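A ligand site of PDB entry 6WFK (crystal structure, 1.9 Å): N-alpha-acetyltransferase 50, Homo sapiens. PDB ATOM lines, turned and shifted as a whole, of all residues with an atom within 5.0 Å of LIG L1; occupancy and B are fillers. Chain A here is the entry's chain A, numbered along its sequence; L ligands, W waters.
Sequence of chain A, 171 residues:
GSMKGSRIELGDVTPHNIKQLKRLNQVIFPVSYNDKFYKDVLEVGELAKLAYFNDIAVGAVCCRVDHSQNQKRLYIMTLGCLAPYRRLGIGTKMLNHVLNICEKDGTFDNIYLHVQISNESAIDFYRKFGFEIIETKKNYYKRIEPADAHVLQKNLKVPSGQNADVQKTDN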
ATOM      1  N   ILE A  28     -24.425 -13.561 -30.706  1.00  0.00           N
ATOM      2  CA  ILE A  28     -23.030 -13.132 -30.840  1.00  0.00           C
ATOM      3  C   ILE A  28     -22.003 -14.204 -30.433  1.00  0.00           C
ATOM      4  O   ILE A  28     -20.959 -14.291 -31.062  1.00  0.00           O
ATOM      5  CB  ILE A  28     -22.802 -11.771 -30.062  1.00  0.00           C
ATOM      6  CG1 ILE A  28     -23.627 -10.632 -30.701  1.00  0.00           C
ATOM      7  CG2 ILE A  28     -21.307 -11.378 -29.979  1.00  0.00           C
ATOM      8  CD1 ILE A  28     -23.952  -9.460 -29.729  1.00  0.00           C
ATOM      9  N   PHE A  29     -22.278 -14.940 -29.356  1.00  0.00           N
ATOM     10  CA  PHE A  29     -21.301 -15.869 -28.794  1.00  0.00           C
ATOM     11  C   PHE A  29     -21.517 -17.330 -29.143  1.00  0.00           C
ATOM     12  O   PHE A  29     -22.662 -17.792 -29.226  1.00  0.00           O
ATOM     13  CB  PHE A  29     -21.181 -15.665 -27.278  1.00  0.00           C
ATOM     14  CG  PHE A  29     -20.720 -14.246 -26.963  1.00  0.00           C
ATOM     15  CD1 PHE A  29     -19.448 -13.807 -27.344  1.00  0.00           C
ATOM     16  CD2 PHE A  29     -21.594 -13.328 -26.381  1.00  0.00           C
ATOM     17  CE1 PHE A  29     -19.044 -12.496 -27.106  1.00  0.00           C
ATOM     18  CE2 PHE A  29     -21.183 -12.012 -26.131  1.00  0.00           C
ATOM     19  CZ  PHE A  29     -19.903 -11.617 -26.485  1.00  0.00           C
ATOM     20  N   ILE A  76     -13.706  -9.430 -17.620  1.00  0.00           N
ATOM     21  CA  ILE A  76     -14.709  -9.198 -18.675  1.00  0.00           C
ATOM     22  C   ILE A  76     -15.117 -10.567 -19.127  1.00  0.00           C
ATOM     23  O   ILE A  76     -14.292 -11.290 -19.680  1.00  0.00           O
ATOM     24  CB  ILE A  76     -14.184  -8.366 -19.869  1.00  0.00           C
ATOM     25  CG1 ILE A  76     -13.618  -7.003 -19.401  1.00  0.00           C
ATOM     26  CG2 ILE A  76     -15.261  -8.241 -20.984  1.00  0.00           C
ATOM     27  CD1 ILE A  76     -12.768  -6.271 -20.510  1.00  0.00           C
ATOM     28  N   MET A  77     -16.392 -10.919 -18.899  1.00  0.00           N
ATOM     29  CA  MET A  77     -16.915 -12.233 -19.281  1.00  0.00           C
ATOM     30  C   MET A  77     -17.359 -12.234 -20.723  1.00  0.00           C
ATOM     31  O   MET A  77     -17.042 -13.166 -21.467  1.00  0.00           O
ATOM     32  CB  MET A  77     -18.053 -12.671 -18.354  1.00  0.00           C
ATOM     33  CG  MET A  77     -17.593 -12.898 -16.922  1.00  0.00           C
ATOM     34  SD  MET A  77     -18.949 -13.305 -15.803  1.00  0.00           S
ATOM     35  CE  MET A  77     -19.703 -11.722 -15.638  1.00  0.00           C
ATOM     36  N   THR A  78     -18.102 -11.203 -21.127  1.00  0.00           N
ATOM     37  CA  THR A  78     -18.589 -11.055 -22.493  1.00  0.00           C
ATOM     38  C   THR A  78     -18.557  -9.588 -22.883  1.00  0.00           C
ATOM     39  O   THR A  78     -18.902  -8.711 -22.081  1.00  0.00           O
ATOM     40  CB  THR A  78     -20.031 -11.590 -22.659  1.00  0.00           C
ATOM     41  OG1 THR A  78     -20.856 -10.961 -21.699  1.00  0.00           O
ATOM     42  CG2 THR A  78     -20.156 -13.099 -22.548  1.00  0.00           C
ATOM     43  N   LEU A  79     -18.178  -9.317 -24.131  1.00  0.00           N
ATOM     44  CA  LEU A  79     -18.174  -7.982 -24.689  1.00  0.00           C
ATOM     45  C   LEU A  79     -18.362  -8.245 -26.174  1.00  0.00           C
ATOM     46  O   LEU A  79     -17.536  -8.893 -26.819  1.00  0.00           O
ATOM     47  CB  LEU A  79     -16.843  -7.225 -24.377  1.00  0.00           C
ATOM     48  CG  LEU A  79     -16.784  -5.706 -24.673  1.00  0.00           C
ATOM     49  CD1 LEU A  79     -15.740  -5.021 -23.797  1.00  0.00           C
ATOM     50  CD2 LEU A  79     -16.460  -5.393 -26.181  1.00  0.00           C
ATOM     51  N   GLY A  80     -19.498  -7.803 -26.700  1.00  0.00           N
ATOM     52  CA  GLY A  80     -19.745  -8.047 -28.101  1.00  0.00           C
ATOM     53  C   GLY A  80     -20.777  -7.152 -28.698  1.00  0.00           C
ATOM     54  O   GLY A  80     -21.569  -6.543 -27.992  1.00  0.00           O
ATOM     55  N   CYS A  81     -20.821  -7.181 -30.012  1.00  0.00           N
ATOM     56  CA  CYS A  81     -21.624  -6.345 -30.865  1.00  0.00           C
ATOM     57  C   CYS A  81     -22.101  -7.237 -32.029  1.00  0.00           C
ATOM     58  O   CYS A  81     -21.330  -8.021 -32.549  1.00  0.00           O
ATOM     59  CB  CYS A  81     -20.682  -5.223 -31.349  1.00  0.00           C
ATOM     60  SG  CYS A  81     -21.362  -4.104 -32.570  1.00  0.00           S
ATOM     61  N   TYR A  85     -23.130  -4.267 -37.108  1.00  0.00           N
ATOM     62  CA  TYR A  85     -22.824  -2.996 -36.452  1.00  0.00           C
ATOM     63  C   TYR A  85     -21.367  -2.890 -35.986  1.00  0.00           C
ATOM     64  O   TYR A  85     -21.024  -1.942 -35.278  1.00  0.00           O
ATOM     65  CB  TYR A  85     -23.800  -2.759 -35.298  1.00  0.00           C
ATOM     66  CG  TYR A  85     -25.232  -2.681 -35.754  1.00  0.00           C
ATOM     67  CD1 TYR A  85     -25.774  -1.469 -36.210  1.00  0.00           C
ATOM     68  CD2 TYR A  85     -26.053  -3.807 -35.752  1.00  0.00           C
ATOM     69  CE1 TYR A  85     -27.088  -1.398 -36.676  1.00  0.00           C
ATOM     70  CE2 TYR A  85     -27.373  -3.740 -36.189  1.00  0.00           C
ATOM     71  CZ  TYR A  85     -27.882  -2.530 -36.670  1.00  0.00           C
ATOM     72  OH  TYR A  85     -29.198  -2.449 -37.064  1.00  0.00           O
ATOM     73  N   ARG A  86     -20.526  -3.859 -36.366  1.00  0.00           N
ATOM     74  CA  ARG A  86     -19.120  -3.867 -35.987  1.00  0.00           C
ATOM     75  C   ARG A  86     -18.354  -2.735 -36.706  1.00  0.00           C
ATOM     76  O   ARG A  86     -18.835  -2.197 -37.718  1.00  0.00           O
ATOM     77  CB  ARG A  86     -18.495  -5.246 -36.207  1.00  0.00           C
ATOM     78  CG  ARG A  86     -18.803  -6.174 -35.051  1.00  0.00           C
ATOM     79  CD  ARG A  86     -18.476  -7.615 -35.332  1.00  0.00           C
ATOM     80  NE  ARG A  86     -19.365  -8.459 -34.532  1.00  0.00           N
ATOM     81  CZ  ARG A  86     -19.418  -9.785 -34.587  1.00  0.00           C
ATOM     82  NH1 ARG A  86     -18.598 -10.457 -35.380  1.00  0.00           N
ATOM     83  NH2 ARG A  86     -20.300 -10.444 -33.852  1.00  0.00           N
ATOM     84  N   ARG A  87     -17.202  -2.353 -36.141  1.00  0.00           N
ATOM     85  CA  ARG A  87     -16.341  -1.295 -36.669  1.00  0.00           C
ATOM     86  C   ARG A  87     -17.033   0.060 -36.731  1.00  0.00           C
ATOM     87  O   ARG A  87     -16.763   0.848 -37.637  1.00  0.00           O
ATOM     88  CB  ARG A  87     -15.681  -1.638 -38.027  1.00  0.00           C
ATOM     89  CG  ARG A  87     -14.988  -2.987 -38.119  1.00  0.00           C
ATOM     90  CD  ARG A  87     -13.815  -3.093 -37.179  1.00  0.00           C
ATOM     91  NE  ARG A  87     -12.690  -2.224 -37.554  1.00  0.00           N
ATOM     92  CZ  ARG A  87     -11.740  -2.558 -38.419  1.00  0.00           C
ATOM     93  NH1 ARG A  87     -11.780  -3.728 -39.034  1.00  0.00           N
ATOM     94  NH2 ARG A  87     -10.748  -1.720 -38.679  1.00  0.00           N
ATOM     95  N   LEU A  88     -17.922   0.346 -35.749  1.00  0.00           N
ATOM     96  CA  LEU A  88     -18.580   1.635 -35.640  1.00  0.00           C
ATOM     97  C   LEU A  88     -18.196   2.281 -34.311  1.00  0.00           C
ATOM     98  O   LEU A  88     -18.653   3.373 -34.020  1.00  0.00           O
ATOM     99  CB  LEU A  88     -20.120   1.514 -35.805  1.00  0.00           C
ATOM    100  CG  LEU A  88     -20.660   1.162 -37.221  1.00  0.00           C
ATOM    101  CD1 LEU A  88     -22.159   0.979 -37.203  1.00  0.00           C
ATOM    102  CD2 LEU A  88     -20.234   2.200 -38.270  1.00  0.00           C
ATOM    103  N   GLY A  89     -17.343   1.623 -33.527  1.00  0.00           N
ATOM    104  CA  GLY A  89     -16.902   2.141 -32.238  1.00  0.00           C
ATOM    105  C   GLY A  89     -17.742   1.653 -31.071  1.00  0.00           C
ATOM    106  O   GLY A  89     -17.561   2.112 -29.938  1.00  0.00           O
ATOM    107  N   ILE A  90     -18.622   0.699 -31.311  1.00  0.00           N
ATOM    108  CA  ILE A  90     -19.493   0.134 -30.252  1.00  0.00           C
ATOM    109  C   ILE A  90     -18.656  -0.625 -29.209  1.00  0.00           C
ATOM    110  O   ILE A  90     -18.771  -0.338 -28.019  1.00  0.00           O
ATOM    111  CB  ILE A  90     -20.691  -0.673 -30.804  1.00  0.00           C
ATOM    112  CG1 ILE A  90     -21.645   0.265 -31.565  1.00  0.00           C
ATOM    113  CG2 ILE A  90     -21.440  -1.412 -29.636  1.00  0.00           C
ATOM    114  CD1 ILE A  90     -22.458  -0.359 -32.628  1.00  0.00           C
ATOM    115  N   GLY A  91     -17.767  -1.525 -29.663  1.00  0.00           N
ATOM    116  CA  GLY A  91     -16.871  -2.241 -28.767  1.00  0.00           C
ATOM    117  C   GLY A  91     -16.036  -1.297 -27.921  1.00  0.00           C
ATOM    118  O   GLY A  91     -15.928  -1.511 -26.713  1.00  0.00           O
ATOM    119  N   THR A  92     -15.427  -0.234 -28.575  1.00  0.00           N
ATOM    120  CA  THR A  92     -14.607   0.801 -27.894  1.00  0.00           C
ATOM    121  C   THR A  92     -15.396   1.545 -26.798  1.00  0.00           C
ATOM    122  O   THR A  92     -14.882   1.793 -25.719  1.00  0.00           O
ATOM    123  CB  THR A  92     -14.050   1.828 -28.900  1.00  0.00           C
ATOM    124  OG1 THR A  92     -13.231   1.134 -29.819  1.00  0.00           O
ATOM    125  CG2 THR A  92     -13.270   2.956 -28.253  1.00  0.00           C
ATOM    126  N   LEU A 113      -9.560 -11.107 -19.540  1.00  0.00           N
ATOM    127  CA  LEU A 113     -10.608 -11.860 -20.231  1.00  0.00           C
ATOM    128  C   LEU A 113     -10.006 -13.035 -21.000  1.00  0.00           C
ATOM    129  O   LEU A 113      -8.786 -13.102 -21.195  1.00  0.00           O
ATOM    130  CB  LEU A 113     -11.373 -10.924 -21.196  1.00  0.00           C
ATOM    131  CG  LEU A 113     -10.645 -10.483 -22.471  1.00  0.00           C
ATOM    132  CD1 LEU A 113     -11.607 -10.378 -23.599  1.00  0.00           C
ATOM    133  CD2 LEU A 113      -9.843  -9.184 -22.268  1.00  0.00           C
ATOM    134  N   HIS A 114     -10.876 -13.953 -21.459  1.00  0.00           N
ATOM    135  CA  HIS A 114     -10.491 -15.065 -22.298  1.00  0.00           C
ATOM    136  C   HIS A 114     -10.942 -14.784 -23.711  1.00  0.00           C
ATOM    137  O   HIS A 114     -12.037 -14.253 -23.920  1.00  0.00           O
ATOM    138  CB  HIS A 114     -11.039 -16.408 -21.787  1.00  0.00           C
ATOM    139  CG  HIS A 114     -10.357 -16.868 -20.533  1.00  0.00           C
ATOM    140  ND1 HIS A 114     -10.746 -16.403 -19.294  1.00  0.00           N
ATOM    141  CD2 HIS A 114      -9.289 -17.691 -20.380  1.00  0.00           C
ATOM    142  CE1 HIS A 114      -9.934 -16.983 -18.414  1.00  0.00           C
ATOM    143  NE2 HIS A 114      -9.049 -17.773 -19.027  1.00  0.00           N
ATOM    144  N   VAL A 115     -10.082 -15.078 -24.699  1.00  0.00           N
ATOM    145  CA  VAL A 115     -10.421 -14.879 -26.104  1.00  0.00           C
ATOM    146  C   VAL A 115     -10.048 -16.170 -26.828  1.00  0.00           C
ATOM    147  O   VAL A 115      -8.864 -16.541 -26.837  1.00  0.00           O
ATOM    148  CB  VAL A 115      -9.692 -13.653 -26.775  1.00  0.00           C
ATOM    149  CG1 VAL A 115     -10.117 -13.509 -28.224  1.00  0.00           C
ATOM    150  CG2 VAL A 115      -9.937 -12.351 -26.007  1.00  0.00           C
ATOM    151  N   ASN A 119     -10.231 -16.081 -32.733  1.00  0.00           N
ATOM    152  CA  ASN A 119     -10.804 -14.745 -32.786  1.00  0.00           C
ATOM    153  C   ASN A 119      -9.743 -13.672 -32.959  1.00  0.00           C
ATOM    154  O   ASN A 119      -9.480 -12.867 -32.060  1.00  0.00           O
ATOM    155  CB  ASN A 119     -11.677 -14.490 -31.560  1.00  0.00           C
ATOM    156  CG  ASN A 119     -12.730 -13.462 -31.855  1.00  0.00           C
ATOM    157  OD1 ASN A 119     -12.609 -12.605 -32.737  1.00  0.00           O
ATOM    158  ND2 ASN A 119     -13.786 -13.541 -31.098  1.00  0.00           N
ATOM    159  N   SER A 121      -9.778 -10.893 -34.814  1.00  0.00           N
ATOM    160  CA  SER A 121     -10.333  -9.549 -34.720  1.00  0.00           C
ATOM    161  C   SER A 121     -10.476  -9.097 -33.235  1.00  0.00           C
ATOM    162  O   SER A 121     -10.171  -7.935 -32.944  1.00  0.00           O
ATOM    163  CB  SER A 121     -11.650  -9.447 -35.480  1.00  0.00           C
ATOM    164  OG  SER A 121     -12.809  -9.667 -34.680  1.00  0.00           O
ATOM    165  N   ALA A 122     -10.892 -10.005 -32.310  1.00  0.00           N
ATOM    166  CA  ALA A 122     -10.988  -9.653 -30.892  1.00  0.00           C
ATOM    167  C   ALA A 122      -9.601  -9.440 -30.290  1.00  0.00           C
ATOM    168  O   ALA A 122      -9.447  -8.511 -29.515  1.00  0.00           O
ATOM    169  CB  ALA A 122     -11.770 -10.714 -30.105  1.00  0.00           C
ATOM    170  N   ASP A 124      -6.858  -8.361 -31.920  1.00  0.00           N
ATOM    171  CA  ASP A 124      -6.486  -7.060 -32.489  1.00  0.00           C
ATOM    172  C   ASP A 124      -7.085  -5.908 -31.681  1.00  0.00           C
ATOM    173  O   ASP A 124      -6.404  -4.930 -31.391  1.00  0.00           O
ATOM    174  CB  ASP A 124      -7.019  -6.929 -33.917  1.00  0.00           C
ATOM    175  CG  ASP A 124      -5.987  -7.106 -35.012  1.00  0.00           C
ATOM    176  OD1 ASP A 124      -4.871  -6.545 -34.879  1.00  0.00           O
ATOM    177  OD2 ASP A 124      -6.312  -7.771 -36.015  1.00  0.00           O
ATOM    178  N   PHE A 125      -8.411  -5.995 -31.445  1.00  0.00           N
ATOM    179  CA  PHE A 125      -9.218  -5.037 -30.712  1.00  0.00           C
ATOM    180  C   PHE A 125      -8.622  -4.780 -29.319  1.00  0.00           C
ATOM    181  O   PHE A 125      -8.279  -3.654 -28.996  1.00  0.00           O
ATOM    182  CB  PHE A 125     -10.698  -5.508 -30.660  1.00  0.00           C
ATOM    183  CG  PHE A 125     -11.582  -4.702 -29.726  1.00  0.00           C
ATOM    184  CD1 PHE A 125     -12.059  -3.449 -30.113  1.00  0.00           C
ATOM    185  CD2 PHE A 125     -11.899  -5.172 -28.455  1.00  0.00           C
ATOM    186  CE1 PHE A 125     -12.835  -2.690 -29.239  1.00  0.00           C
ATOM    187  CE2 PHE A 125     -12.697  -4.415 -27.585  1.00  0.00           C
ATOM    188  CZ  PHE A 125     -13.153  -3.173 -27.980  1.00  0.00           C
ATOM    189  N   TYR A 126      -8.444  -5.834 -28.526  1.00  0.00           N
ATOM    190  CA  TYR A 126      -7.925  -5.673 -27.161  1.00  0.00           C
ATOM    191  C   TYR A 126      -6.470  -5.211 -27.096  1.00  0.00           C
ATOM    192  O   TYR A 126      -6.138  -4.382 -26.242  1.00  0.00           O
ATOM    193  CB  TYR A 126      -8.146  -6.941 -26.366  1.00  0.00           C
ATOM    194  CG  TYR A 126      -9.598  -7.151 -26.005  1.00  0.00           C
ATOM    195  CD1 TYR A 126     -10.206  -6.404 -25.000  1.00  0.00           C
ATOM    196  CD2 TYR A 126     -10.370  -8.094 -26.675  1.00  0.00           C
ATOM    197  CE1 TYR A 126     -11.553  -6.592 -24.670  1.00  0.00           C
ATOM    198  CE2 TYR A 126     -11.711  -8.276 -26.383  1.00  0.00           C
ATOM    199  CZ  TYR A 126     -12.299  -7.529 -25.365  1.00  0.00           C
ATOM    200  OH  TYR A 126     -13.610  -7.764 -25.055  1.00  0.00           O
ATOM    201  N   LYS A 128      -5.028  -3.216 -29.100  1.00  0.00           N
ATOM    202  CA  LYS A 128      -5.078  -1.782 -29.376  1.00  0.00           C
ATOM    203  C   LYS A 128      -5.287  -0.974 -28.046  1.00  0.00           C
ATOM    204  O   LYS A 128      -4.827   0.150 -27.928  1.00  0.00           O
ATOM    205  CB  LYS A 128      -6.216  -1.520 -30.369  1.00  0.00           C
ATOM    206  CG  LYS A 128      -6.273  -0.129 -30.970  1.00  0.00           C
ATOM    207  CD  LYS A 128      -7.728   0.332 -31.170  1.00  0.00           C
ATOM    208  CE  LYS A 128      -7.818   1.657 -31.899  1.00  0.00           C
ATOM    209  NZ  LYS A 128      -7.583   1.505 -33.366  1.00  0.00           N
ATOM    210  N   PHE A 129      -5.934  -1.582 -27.037  1.00  0.00           N
ATOM    211  CA  PHE A 129      -6.190  -0.947 -25.751  1.00  0.00           C
ATOM    212  C   PHE A 129      -5.104  -1.220 -24.717  1.00  0.00           C
ATOM    213  O   PHE A 129      -5.259  -0.839 -23.562  1.00  0.00           O
ATOM    214  CB  PHE A 129      -7.582  -1.337 -25.221  1.00  0.00           C
ATOM    215  CG  PHE A 129      -8.681  -0.662 -25.994  1.00  0.00           C
ATOM    216  CD1 PHE A 129      -9.146  -1.197 -27.198  1.00  0.00           C
ATOM    217  CD2 PHE A 129      -9.288   0.494 -25.526  1.00  0.00           C
ATOM    218  CE1 PHE A 129     -10.153  -0.570 -27.922  1.00  0.00           C
ATOM    219  CE2 PHE A 129     -10.319   1.118 -26.243  1.00  0.00           C
ATOM    220  CZ  PHE A 129     -10.749   0.581 -27.441  1.00  0.00           C
HETATM  221  N1  LIG L   1      -9.736  -6.284 -37.830  1.00  0.00           N
HETATM  222  C1  LIG L   1      -8.757  -5.485 -37.400  1.00  0.00           C
HETATM  223  N2  LIG L   1      -8.767  -4.635 -36.368  1.00  0.00           N
HETATM  224  C2  LIG L   1      -9.955  -4.642 -35.748  1.00  0.00           C
HETATM  225  C3  LIG L   1     -11.052  -5.400 -36.110  1.00  0.00           C
HETATM  226  C4  LIG L   1     -10.916  -6.250 -37.202  1.00  0.00           C
HETATM  227  N3  LIG L   1     -11.980  -7.044 -37.646  1.00  0.00           N
HETATM  228  N4  LIG L   1     -12.111  -5.149 -35.276  1.00  0.00           N
HETATM  229  C5  LIG L   1     -11.660  -4.254 -34.433  1.00  0.00           C
HETATM  230  N5  LIG L   1     -10.353  -3.916 -34.658  1.00  0.00           N
HETATM  231  C6  LIG L   1      -9.616  -2.840 -33.995  1.00  0.00           C
HETATM  232  C7  LIG L   1      -9.487  -1.630 -34.897  1.00  0.00           C
HETATM  233  O1  LIG L   1      -8.271  -0.920 -34.725  1.00  0.00           O
HETATM  234  C8  LIG L   1     -10.700  -0.810 -34.501  1.00  0.00           C
HETATM  235  O2  LIG L   1     -10.549   0.578 -34.779  1.00  0.00           O
HETATM  236  P1  LIG L   1     -11.054   1.112 -36.237  1.00  0.00           P
HETATM  237  O3  LIG L   1     -11.047   2.607 -36.053  1.00  0.00           O
HETATM  238  O4  LIG L   1      -9.984   0.596 -37.199  1.00  0.00           O
HETATM  239  O5  LIG L   1     -12.421   0.483 -36.454  1.00  0.00           O
HETATM  240  C9  LIG L   1     -10.759  -1.032 -33.015  1.00  0.00           C
HETATM  241  O6  LIG L   1     -10.324  -2.379 -32.834  1.00  0.00           O
HETATM  242  C10 LIG L   1     -12.120  -0.734 -32.402  1.00  0.00           C
HETATM  243  O7  LIG L   1     -13.219  -1.304 -33.118  1.00  0.00           O
HETATM  244  P2  LIG L   1     -14.743  -0.929 -32.676  1.00  0.00           P
HETATM  245  O8  LIG L   1     -15.553  -0.507 -33.865  1.00  0.00           O
HETATM  246  O9  LIG L   1     -14.804  -0.179 -31.390  1.00  0.00           O
HETATM  247  O10 LIG L   1     -15.123  -2.470 -32.265  1.00  0.00           O
HETATM  248  P3  LIG L   1     -16.424  -3.400 -32.545  1.00  0.00           P
HETATM  249  O11 LIG L   1     -17.662  -2.656 -32.144  1.00  0.00           O
HETATM  250  O12 LIG L   1     -16.307  -3.895 -33.969  1.00  0.00           O
HETATM  251  O13 LIG L   1     -16.112  -4.496 -31.375  1.00  0.00           O
HETATM  252  C11 LIG L   1     -15.521  -6.787 -30.952  1.00  0.00           C
HETATM  253  C12 LIG L   1     -15.020  -5.417 -31.396  1.00  0.00           C
HETATM  254  C13 LIG L   1     -14.321  -7.680 -30.756  1.00  0.00           C
HETATM  255  C14 LIG L   1     -16.190  -6.642 -29.583  1.00  0.00           C
HETATM  256  C15 LIG L   1     -16.476  -7.337 -32.029  1.00  0.00           C
HETATM  257  O14 LIG L   1     -15.793  -7.754 -33.199  1.00  0.00           O
HETATM  258  C16 LIG L   1     -17.410  -8.452 -31.635  1.00  0.00           C
HETATM  259  O15 LIG L   1     -18.536  -8.197 -31.242  1.00  0.00           O
HETATM  260  N6  LIG L   1     -16.960  -9.743 -31.781  1.00  0.00           N
HETATM  261  C17 LIG L   1     -17.605 -10.844 -31.087  1.00  0.00           C
HETATM  262  C18 LIG L   1     -17.396 -10.748 -29.591  1.00  0.00           C
HETATM  263  C19 LIG L   1     -16.078 -11.340 -29.249  1.00  0.00           C
HETATM  264  O16 LIG L   1     -15.611 -12.161 -30.002  1.00  0.00           O
HETATM  265  N7  LIG L   1     -15.480 -10.944 -28.062  1.00  0.00           N
HETATM  266  C20 LIG L   1     -14.761 -11.952 -27.301  1.00  0.00           C
HETATM  267  C21 LIG L   1     -14.116 -11.431 -26.047  1.00  0.00           C
HETATM  268  S1  LIG L   1     -15.412 -11.252 -24.793  1.00  0.00           S
HETATM  269  C1  LG2 L   2     -18.568 -21.680 -21.556  1.00  0.00           C
HETATM  270  C2  LG2 L   2     -16.422 -22.696 -21.262  1.00  0.00           C
HETATM  271  C3  LG2 L   2     -18.240 -20.700 -20.640  1.00  0.00           C
HETATM  272  C4  LG2 L   2     -16.087 -21.723 -20.357  1.00  0.00           C
HETATM  273  C5  LG2 L   2     -19.454 -17.147 -16.061  1.00  0.00           C
HETATM  274  C6  LG2 L   2     -17.665 -22.682 -21.858  1.00  0.00           C
HETATM  275  C7  LG2 L   2     -16.993 -20.735 -20.057  1.00  0.00           C
HETATM  276  C8  LG2 L   2     -18.263 -16.982 -15.387  1.00  0.00           C
HETATM  277  C9  LG2 L   2     -18.035 -23.712 -22.859  1.00  0.00           C
HETATM  278  C10 LG2 L   2     -17.446 -17.216 -17.409  1.00  0.00           C
HETATM  279  C11 LG2 L   2     -16.962 -15.981 -25.566  1.00  0.00           C
HETATM  280  C12 LG2 L   2     -14.608 -15.700 -26.137  1.00  0.00           C
HETATM  281  C13 LG2 L   2     -16.649 -19.710 -19.081  1.00  0.00           C
HETATM  282  C14 LG2 L   2     -18.177 -16.785 -13.950  1.00  0.00           C
HETATM  283  C15 LG2 L   2     -15.333 -15.941 -22.946  1.00  0.00           C
HETATM  284  C16 LG2 L   2     -16.782 -14.824 -24.621  1.00  0.00           C
HETATM  285  C17 LG2 L   2     -16.418 -16.057 -19.350  1.00  0.00           C
HETATM  286  C18 LG2 L   2     -16.539 -17.879 -20.821  1.00  0.00           C
HETATM  287  C19 LG2 L   2     -16.475 -17.314 -18.514  1.00  0.00           C
HETATM  288  C20 LG2 L   2     -15.422 -14.823 -23.951  1.00  0.00           C
HETATM  289  C21 LG2 L   2     -15.801 -16.574 -20.628  1.00  0.00           C
HETATM  290  C22 LG2 L   2     -15.876 -17.523 -27.113  1.00  0.00           C
HETATM  291  C23 LG2 L   2     -16.580 -16.865 -12.060  1.00  0.00           C
HETATM  292  N1  LG2 L   2     -17.153 -24.553 -23.429  1.00  0.00           N
HETATM  293  N2  LG2 L   2     -17.123 -17.026 -16.157  1.00  0.00           N
HETATM  294  N3  LG2 L   2     -19.286 -23.861 -23.347  1.00  0.00           N
HETATM  295  N4  LG2 L   2     -17.884 -25.259 -24.325  1.00  0.00           N
HETATM  296  N5  LG2 L   2     -19.181 -24.843 -24.278  1.00  0.00           N
HETATM  297  N6  LG2 L   2     -14.411 -15.005 -24.958  1.00  0.00           N
HETATM  298  N7  LG2 L   2     -15.816 -16.384 -26.222  1.00  0.00           N
HETATM  299  N8  LG2 L   2     -16.726 -18.373 -19.478  1.00  0.00           N
HETATM  300  N9  LG2 L   2     -16.910 -17.019 -13.463  1.00  0.00           N
HETATM  301  N10 LG2 L   2     -15.935 -15.663 -21.741  1.00  0.00           N
HETATM  302  O1  LG2 L   2     -18.062 -16.508 -25.701  1.00  0.00           O
HETATM  303  O2  LG2 L   2     -13.792 -15.714 -27.052  1.00  0.00           O
HETATM  304  O3  LG2 L   2     -16.338 -20.087 -17.963  1.00  0.00           O
HETATM  305  O4  LG2 L   2     -19.149 -16.449 -13.283  1.00  0.00           O
HETATM  306  O5  LG2 L   2     -14.795 -17.017 -23.169  1.00  0.00           O
HETATM  307  S1  LG2 L   2     -19.124 -17.375 -17.737  1.00  0.00           S
HETATM  308  O   HOH W   1     -14.814 -11.090 -33.421  1.00  0.00           O
HETATM  309  O   HOH W   2     -14.830  -5.695 -35.073  1.00  0.00           O
HETATM  310  O   HOH W   3     -15.305  -7.030 -37.449  1.00  0.00           O
HETATM  311  O   HOH W   4     -19.036  -1.135 -33.665  1.00  0.00           O
HETATM  312  O   HOH W   5     -10.840   2.100 -30.911  1.00  0.00           O
HETATM  313  O   HOH W   6     -14.129   1.750 -34.974  1.00  0.00           O
HETATM  314  O   HOH W   7     -17.063 -14.805 -29.445  1.00  0.00           O
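A nitrogen (N10) of LG2 L2 sits at hydrogen-bond distance from the backbone carbonyl oxygen (O) of Met 77 (2.7 Å).
The backbone NH of Gly 89 is in hydrogen-bond range of an oxygen (O8) of LIG L1.
The backbone NH of Thr 92 sits at hydrogen-bond distance from an oxygen (O9) of LIG L1 (2.9 Å).
The guanidinium group of Arg 86 sits at hydrogen-bond distance from an oxygen (O15) of LIG L1, 3.4 Å away.
The guanidinium group (NH2) of Arg 87 lies within salt-bridge range of an oxygen (O4) of LIG L1 (2.9 Å).
The backbone carbonyl oxygen (O) of His 114 is in hydrogen-bond range of a nitrogen (N6) of LG2 L2, 2.7 Å away.
N of Arg 87 lies within hydrogen-bond range of O12 of LIG L1, at 2.8 Å.
The backbone carbonyl oxygen (O) of Leu 79 sits at hydrogen-bond distance from a nitrogen (N7) of LIG L1, at 3.2 Å.
N of Cys 81 is in hydrogen-bond range of O15 of LIG L1 (2.8 Å).
The side-chain hydroxyl of Thr 92 is in hydrogen-bond range of an oxygen (O9) of LIG L1 (2.6 Å).
O8 of LIG L1 is in hydrogen-bond range of N of Leu 88 (3.1 Å).
The side-chain amide nitrogen (ND2) of Asn 119 is in hydrogen-bond range of an oxygen (O16) of LIG L1, 2.5 Å away.
An oxygen (O11) of LIG L1 is in hydrogen-bond range of the backbone NH of Gly 91, 2.7 Å away.
The backbone NH of Leu 79 lies close to a sulfur (S1) of LIG L1.
NZ of Lys 128 is in hydrogen-bond range of O1 of LIG L1 (2.9 Å).
The guanidinium group of Arg 86 sits at hydrogen-bond distance from the backbone carbonyl oxygen of Cys 81, 2.8 Å away.
The backbone carbonyl oxygen of Tyr 85 is in hydrogen-bond range of the side-chain sulfur of Cys 81 (3.5 Å).
OD1 of Asn 119 lies within hydrogen-bond range of N of Ala 122 (3.1 Å).
CG2 of Ile 28 touches C17 of LIG L1, 3.9 Å away.
Phe 29 touches LIG L1.
Thr 78 touches LIG L1 (CA to S1, 3.9 Å).
CA of Gly 80 touches O15 of LIG L1, at 3.4 Å.
Ile 90 touches LIG L1 (N to O11, 3.6 Å).
CD1 of Leu 113 touches C21 of LIG L1, 3.7 Å away.
Ser 121 touches LIG L1.
Ala 122 touches LIG L1 (CA to C13, 3.9 Å).
OD2 of Asp 124 touches C1 of LIG L1 (3.6 Å).
Phe 125 touches LIG L1 (CD1 to O6, 3.4 Å).
Tyr 126 touches LIG L1 (OH to C21, 3.8 Å).
Of the 27 residues printed, 21 come within 4 Å of LIG L1.
Water W1 lies within hydrogen-bond range of OD1 of Asn 119 (2.8 Å), OG of Ser 121 (2.8 Å) and N6 of LIG L1 (3.0 Å).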
